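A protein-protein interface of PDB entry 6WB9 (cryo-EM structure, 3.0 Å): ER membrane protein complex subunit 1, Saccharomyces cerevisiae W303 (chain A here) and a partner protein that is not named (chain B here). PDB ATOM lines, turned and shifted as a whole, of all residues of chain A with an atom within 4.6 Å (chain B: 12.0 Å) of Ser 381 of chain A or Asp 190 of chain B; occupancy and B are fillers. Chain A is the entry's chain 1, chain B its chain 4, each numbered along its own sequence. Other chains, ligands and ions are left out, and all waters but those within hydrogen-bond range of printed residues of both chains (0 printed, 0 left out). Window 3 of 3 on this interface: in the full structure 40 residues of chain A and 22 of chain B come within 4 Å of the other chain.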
ATOM      1  N   VAL A 334     -17.857 -11.615  -3.884  1.00  0.00           N
ATOM      2  CA  VAL A 334     -19.293 -11.607  -4.151  1.00  0.00           C
ATOM      3  C   VAL A 334     -19.585 -11.372  -5.630  1.00  0.00           C
ATOM      4  O   VAL A 334     -20.174 -12.222  -6.297  1.00  0.00           O
ATOM      5  CB  VAL A 334     -20.014 -10.564  -3.268  1.00  0.00           C
ATOM      6  CG1 VAL A 334     -21.482 -10.486  -3.626  1.00  0.00           C
ATOM      7  CG2 VAL A 334     -19.847 -10.909  -1.801  1.00  0.00           C
ATOM      8  N   VAL A 379     -21.520  -7.405   2.456  1.00  0.00           N
ATOM      9  CA  VAL A 379     -22.104  -7.192   1.134  1.00  0.00           C
ATOM     10  C   VAL A 379     -22.859  -8.446   0.717  1.00  0.00           C
ATOM     11  O   VAL A 379     -22.328  -9.559   0.793  1.00  0.00           O
ATOM     12  CB  VAL A 379     -21.016  -6.827   0.113  1.00  0.00           C
ATOM     13  CG1 VAL A 379     -21.588  -6.736  -1.290  1.00  0.00           C
ATOM     14  CG2 VAL A 379     -20.352  -5.522   0.495  1.00  0.00           C
ATOM     15  N   ASP A 380     -24.106  -8.270   0.280  1.00  0.00           N
ATOM     16  CA  ASP A 380     -24.938  -9.369  -0.196  1.00  0.00           C
ATOM     17  C   ASP A 380     -24.896  -9.516  -1.712  1.00  0.00           C
ATOM     18  O   ASP A 380     -24.597 -10.601  -2.218  1.00  0.00           O
ATOM     19  CB  ASP A 380     -26.383  -9.168   0.271  1.00  0.00           C
ATOM     20  CG  ASP A 380     -27.267 -10.352  -0.056  1.00  0.00           C
ATOM     21  OD1 ASP A 380     -27.092 -11.415   0.576  1.00  0.00           O
ATOM     22  OD2 ASP A 380     -28.137 -10.222  -0.942  1.00  0.00           O
ATOM     23  N   SER A 381     -25.187  -8.446  -2.448  1.00  0.00           N
ATOM     24  CA  SER A 381     -25.127  -8.470  -3.903  1.00  0.00           C
ATOM     25  C   SER A 381     -24.930  -7.051  -4.409  1.00  0.00           C
ATOM     26  O   SER A 381     -25.386  -6.090  -3.789  1.00  0.00           O
ATOM     27  CB  SER A 381     -26.394  -9.079  -4.516  1.00  0.00           C
ATOM     28  OG  SER A 381     -27.529  -8.273  -4.254  1.00  0.00           O
ATOM     29  N   VAL A 382     -24.242  -6.934  -5.543  1.00  0.00           N
ATOM     30  CA  VAL A 382     -23.953  -5.651  -6.172  1.00  0.00           C
ATOM     31  C   VAL A 382     -24.614  -5.627  -7.543  1.00  0.00           C
ATOM     32  O   VAL A 382     -24.572  -6.617  -8.280  1.00  0.00           O
ATOM     33  CB  VAL A 382     -22.434  -5.406  -6.292  1.00  0.00           C
ATOM     34  CG1 VAL A 382     -22.151  -3.973  -6.696  1.00  0.00           C
ATOM     35  CG2 VAL A 382     -21.734  -5.733  -4.987  1.00  0.00           C
ATOM     36  N   ILE A 383     -25.239  -4.498  -7.874  1.00  0.00           N
ATOM     37  CA  ILE A 383     -25.883  -4.284  -9.165  1.00  0.00           C
ATOM     38  C   ILE A 383     -25.181  -3.123  -9.853  1.00  0.00           C
ATOM     39  O   ILE A 383     -25.021  -2.053  -9.260  1.00  0.00           O
ATOM     40  CB  ILE A 383     -27.386  -3.991  -9.003  1.00  0.00           C
ATOM     41  CG1 ILE A 383     -28.069  -5.127  -8.250  1.00  0.00           C
ATOM     42  CG2 ILE A 383     -28.045  -3.792 -10.350  1.00  0.00           C
ATOM     43  CD1 ILE A 383     -29.515  -4.864  -7.962  1.00  0.00           C
ATOM     44  N   LEU A 393     -24.829  -0.433  -6.900  1.00  0.00           N
ATOM     45  CA  LEU A 393     -25.943  -0.436  -5.950  1.00  0.00           C
ATOM     46  C   LEU A 393     -25.731  -1.544  -4.918  1.00  0.00           C
ATOM     47  O   LEU A 393     -26.469  -2.529  -4.880  1.00  0.00           O
ATOM     48  CB  LEU A 393     -27.304  -0.586  -6.616  1.00  0.00           C
ATOM     49  CG  LEU A 393     -28.418  -0.382  -5.583  1.00  0.00           C
ATOM     50  CD1 LEU A 393     -29.623   0.260  -6.217  1.00  0.00           C
ATOM     51  CD2 LEU A 393     -28.785  -1.669  -4.885  1.00  0.00           C
ATOM     52  N   ILE A 394     -24.639  -1.435  -4.163  1.00  0.00           N
ATOM     53  CA  ILE A 394     -24.231  -2.457  -3.203  1.00  0.00           C
ATOM     54  C   ILE A 394     -25.295  -2.689  -2.139  1.00  0.00           C
ATOM     55  O   ILE A 394     -25.589  -1.805  -1.330  1.00  0.00           O
ATOM     56  CB  ILE A 394     -22.900  -2.067  -2.547  1.00  0.00           C
ATOM     57  CG1 ILE A 394     -21.837  -1.878  -3.618  1.00  0.00           C
ATOM     58  CG2 ILE A 394     -22.478  -3.111  -1.541  1.00  0.00           C
ATOM     59  CD1 ILE A 394     -20.551  -1.396  -3.081  1.00  0.00           C
ATOM     60  N   LYS A 395     -25.881  -3.879  -2.149  1.00  0.00           N
ATOM     61  CA  LYS A 395     -26.909  -4.264  -1.195  1.00  0.00           C
ATOM     62  C   LYS A 395     -26.261  -5.065  -0.078  1.00  0.00           C
ATOM     63  O   LYS A 395     -25.469  -5.973  -0.343  1.00  0.00           O
ATOM     64  CB  LYS A 395     -28.001  -5.090  -1.872  1.00  0.00           C
ATOM     65  CG  LYS A 395     -29.098  -5.545  -0.934  1.00  0.00           C
ATOM     66  CD  LYS A 395     -29.809  -6.766  -1.468  1.00  0.00           C
ATOM     67  CE  LYS A 395     -30.873  -7.232  -0.497  1.00  0.00           C
ATOM     68  NZ  LYS A 395     -30.303  -7.521   0.847  1.00  0.00           N
ATOM     69  N   THR A 429     -34.874  -2.920  -9.629  1.00  0.00           N
ATOM     70  CA  THR A 429     -35.672  -3.915  -8.934  1.00  0.00           C
ATOM     71  C   THR A 429     -34.764  -4.986  -8.344  1.00  0.00           C
ATOM     72  O   THR A 429     -33.667  -5.246  -8.842  1.00  0.00           O
ATOM     73  CB  THR A 429     -36.713  -4.539  -9.862  1.00  0.00           C
ATOM     74  OG1 THR A 429     -37.396  -5.591  -9.179  1.00  0.00           O
ATOM     75  CG2 THR A 429     -36.058  -5.105 -11.074  1.00  0.00           C
ATOM     76  N   GLU A 430     -35.219  -5.583  -7.247  1.00  0.00           N
ATOM     77  CA  GLU A 430     -34.421  -6.536  -6.486  1.00  0.00           C
ATOM     78  C   GLU A 430     -35.331  -7.631  -5.965  1.00  0.00           C
ATOM     79  O   GLU A 430     -36.301  -7.347  -5.260  1.00  0.00           O
ATOM     80  CB  GLU A 430     -33.705  -5.858  -5.320  1.00  0.00           C
ATOM     81  CG  GLU A 430     -32.464  -5.096  -5.704  1.00  0.00           C
ATOM     82  CD  GLU A 430     -31.552  -4.877  -4.530  1.00  0.00           C
ATOM     83  OE1 GLU A 430     -31.990  -5.138  -3.391  1.00  0.00           O
ATOM     84  OE2 GLU A 430     -30.397  -4.451  -4.739  1.00  0.00           O
ATOM     85  N   HIS A 431     -35.019  -8.872  -6.298  1.00  0.00           N
ATOM     86  CA  HIS A 431     -35.815  -9.985  -5.819  1.00  0.00           C
ATOM     87  C   HIS A 431     -35.198 -10.584  -4.561  1.00  0.00           C
ATOM     88  O   HIS A 431     -34.000 -10.460  -4.301  1.00  0.00           O
ATOM     89  CB  HIS A 431     -35.950 -11.053  -6.897  1.00  0.00           C
ATOM     90  CG  HIS A 431     -34.666 -11.745  -7.224  1.00  0.00           C
ATOM     91  ND1 HIS A 431     -34.445 -13.074  -6.935  1.00  0.00           N
ATOM     92  CD2 HIS A 431     -33.535 -11.297  -7.817  1.00  0.00           C
ATOM     93  CE1 HIS A 431     -33.234 -13.414  -7.336  1.00  0.00           C
ATOM     94  NE2 HIS A 431     -32.661 -12.353  -7.874  1.00  0.00           N
ATOM     95  N   TYR A 463     -37.026 -16.139 -10.669  1.00  0.00           N
ATOM     96  CA  TYR A 463     -37.055 -14.746 -11.085  1.00  0.00           C
ATOM     97  C   TYR A 463     -36.115 -14.569 -12.264  1.00  0.00           C
ATOM     98  O   TYR A 463     -35.018 -15.131 -12.273  1.00  0.00           O
ATOM     99  CB  TYR A 463     -36.640 -13.815  -9.940  1.00  0.00           C
ATOM    100  CG  TYR A 463     -36.633 -12.349 -10.293  1.00  0.00           C
ATOM    101  CD1 TYR A 463     -37.802 -11.610 -10.275  1.00  0.00           C
ATOM    102  CD2 TYR A 463     -35.451 -11.701 -10.624  1.00  0.00           C
ATOM    103  CE1 TYR A 463     -37.797 -10.277 -10.590  1.00  0.00           C
ATOM    104  CE2 TYR A 463     -35.437 -10.368 -10.942  1.00  0.00           C
ATOM    105  CZ  TYR A 463     -36.612  -9.665 -10.923  1.00  0.00           C
ATOM    106  OH  TYR A 463     -36.598  -8.337 -11.241  1.00  0.00           O
ATOM    107  N   GLN B 186     -33.704   4.564 -16.933  1.00  0.00           N
ATOM    108  CA  GLN B 186     -32.915   3.353 -17.073  1.00  0.00           C
ATOM    109  C   GLN B 186     -33.360   2.352 -16.022  1.00  0.00           C
ATOM    110  O   GLN B 186     -33.802   2.728 -14.936  1.00  0.00           O
ATOM    111  CB  GLN B 186     -31.421   3.632 -16.922  1.00  0.00           C
ATOM    112  CG  GLN B 186     -30.816   4.428 -18.054  1.00  0.00           C
ATOM    113  CD  GLN B 186     -29.403   4.855 -17.754  1.00  0.00           C
ATOM    114  OE1 GLN B 186     -29.178   5.774 -16.970  1.00  0.00           O
ATOM    115  NE2 GLN B 186     -28.439   4.185 -18.369  1.00  0.00           N
ATOM    116  N   TRP B 187     -33.238   1.072 -16.353  1.00  0.00           N
ATOM    117  CA  TRP B 187     -33.719   0.010 -15.487  1.00  0.00           C
ATOM    118  C   TRP B 187     -32.677  -1.091 -15.372  1.00  0.00           C
ATOM    119  O   TRP B 187     -32.187  -1.597 -16.388  1.00  0.00           O
ATOM    120  CB  TRP B 187     -35.034  -0.551 -16.009  1.00  0.00           C
ATOM    121  CG  TRP B 187     -35.515  -1.695 -15.227  1.00  0.00           C
ATOM    122  CD1 TRP B 187     -35.994  -1.669 -13.960  1.00  0.00           C
ATOM    123  CD2 TRP B 187     -35.575  -3.055 -15.655  1.00  0.00           C
ATOM    124  NE1 TRP B 187     -36.347  -2.929 -13.567  1.00  0.00           N
ATOM    125  CE2 TRP B 187     -36.097  -3.801 -14.591  1.00  0.00           C
ATOM    126  CE3 TRP B 187     -35.226  -3.715 -16.835  1.00  0.00           C
ATOM    127  CZ2 TRP B 187     -36.290  -5.171 -14.671  1.00  0.00           C
ATOM    128  CZ3 TRP B 187     -35.422  -5.071 -16.913  1.00  0.00           C
ATOM    129  CH2 TRP B 187     -35.949  -5.785 -15.840  1.00  0.00           C
ATOM    130  N   PHE B 188     -32.347  -1.459 -14.136  1.00  0.00           N
ATOM    131  CA  PHE B 188     -31.350  -2.474 -13.837  1.00  0.00           C
ATOM    132  C   PHE B 188     -31.921  -3.426 -12.798  1.00  0.00           C
ATOM    133  O   PHE B 188     -32.700  -3.022 -11.941  1.00  0.00           O
ATOM    134  CB  PHE B 188     -30.053  -1.832 -13.336  1.00  0.00           C
ATOM    135  CG  PHE B 188     -29.584  -0.702 -14.197  1.00  0.00           C
ATOM    136  CD1 PHE B 188     -28.925  -0.954 -15.386  1.00  0.00           C
ATOM    137  CD2 PHE B 188     -29.833   0.609 -13.839  1.00  0.00           C
ATOM    138  CE1 PHE B 188     -28.511   0.077 -16.190  1.00  0.00           C
ATOM    139  CE2 PHE B 188     -29.420   1.643 -14.643  1.00  0.00           C
ATOM    140  CZ  PHE B 188     -28.763   1.377 -15.819  1.00  0.00           C
ATOM    141  N   SER B 189     -31.558  -4.698 -12.883  1.00  0.00           N
ATOM    142  CA  SER B 189     -32.197  -5.693 -12.038  1.00  0.00           C
ATOM    143  C   SER B 189     -31.165  -6.550 -11.324  1.00  0.00           C
ATOM    144  O   SER B 189     -29.991  -6.600 -11.696  1.00  0.00           O
ATOM    145  CB  SER B 189     -33.138  -6.583 -12.845  1.00  0.00           C
ATOM    146  OG  SER B 189     -33.854  -7.466 -12.002  1.00  0.00           O
ATOM    147  N   ASP B 190     -31.638  -7.233 -10.288  1.00  0.00           N
ATOM    148  CA  ASP B 190     -30.802  -8.074  -9.445  1.00  0.00           C
ATOM    149  C   ASP B 190     -30.424  -9.376 -10.148  1.00  0.00           C
ATOM    150  O   ASP B 190     -30.934  -9.687 -11.225  1.00  0.00           O
ATOM    151  CB  ASP B 190     -31.525  -8.373  -8.130  1.00  0.00           C
ATOM    152  CG  ASP B 190     -30.591  -8.872  -7.048  1.00  0.00           C
ATOM    153  OD1 ASP B 190     -29.677  -8.118  -6.657  1.00  0.00           O
ATOM    154  OD2 ASP B 190     -30.777 -10.014  -6.581  1.00  0.00           O
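Printed residues of chain A that touch a printed residue of chain B: Ser 381, Ile 383, Thr 429, Glu 430, His 431 and Tyr 463. Hydrophobic or aromatic side chains of chain A that line the printed part of chain B: Ile 383, His 431 and Tyr 463. Among the printed residues, no Asp or Glu carboxylate lies within 4 Å of a Lys or Arg side-chain nitrogen of the other chain.
Ile 383 of chain A touches Ser 189 of chain B (CG2 to O, 3.7 Å). Asp 190 of chain B touches Ile 383 of chain A. Thr 429 of chain A touches Trp 187 of chain B. CG2 of Thr 429 of chain A touches OG of Ser 189 of chain B, at 3.4 Å. Glu 430 of chain A touches Asp 190 of chain B.
Of chain B, only Asp 190 (3.2 Å) comes within 4 Å of Ser 381 of chain A. Asp 190 of chain B touches just these residues of chain A: Ser 381 (3.2 Å), Ile 383 (3.5 Å), Thr 429 (3.2 Å), Glu 430 (3.8 Å) and His 431 (3.3 Å). No residue of chain B comes within 4 Å of Val 334 of chain A. No residue of chain B comes within 4 Å of Val 379 of chain A. No residue of chain B comes within 4 Å of Val 382 of chain A. No residue of chain B comes within 4 Å of Ile 394 of chain A. Of chain B, only Trp 187 (3.3 Å), Phe 188 (3.2 Å), Ser 189 (3.4 Å) and Asp 190 (3.2 Å) come within 4 Å of Thr 429 of chain A. Of the printed residues of chain B, Glu 430 of chain A touches Asp 190 (3.8 Å). Printed residues of chain B within 4 Å of His 431 of chain A: Asp 190. Of the printed residues of chain A, Phe 188 of chain B touches Thr 429. Printed residues of chain B within 4 Å of Tyr 463 of chain A: Ser 189 (3.0 Å). Leu 393 of chain A touches none of the printed residues of chain B. Gln 186 of chain B touches none of the printed residues of chain A. The nearest residue of chain B that does not touch Ser 381 of chain A is Ser 189 of chain B (8.0 Å). The nearest printed residue of chain A that does not touch Ser 189 of chain B is Glu 430 of chain A (5.3 Å).
The backbone carbonyl oxygen (O) of Ile 383 of chain A is in hydrogen-bond range of the backbone NH (N) of Leu 393 of chain A (2.9 Å). The backbone NH (N) of Lys 395 of chain A lies within hydrogen-bond range of the backbone carbonyl oxygen (O) of Ser 381 of chain A, at 2.8 Å.
A ring nitrogen (NE2) of His 431 of chain A sits at hydrogen-bond distance from the side-chain carboxylate of Asp 190 of chain B, at 3.3 Å. The backbone carbonyl oxygen (O) of Thr 429 of chain A lies within hydrogen-bond range of the backbone NH (N) of Asp 190 of chain B, 3.2 Å away. The side-chain hydroxyl of Ser 381 of chain A lies within hydrogen-bond range of the side-chain carboxylate of Asp 190 of chain B (3.2 Å). The backbone NH (N) of Thr 429 of chain A is in hydrogen-bond range of the backbone carbonyl oxygen (O) of Phe 188 of chain B. OH of Tyr 463 of chain A is in hydrogen-bond range of OG of Ser 189 of chain B (3.0 Å).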
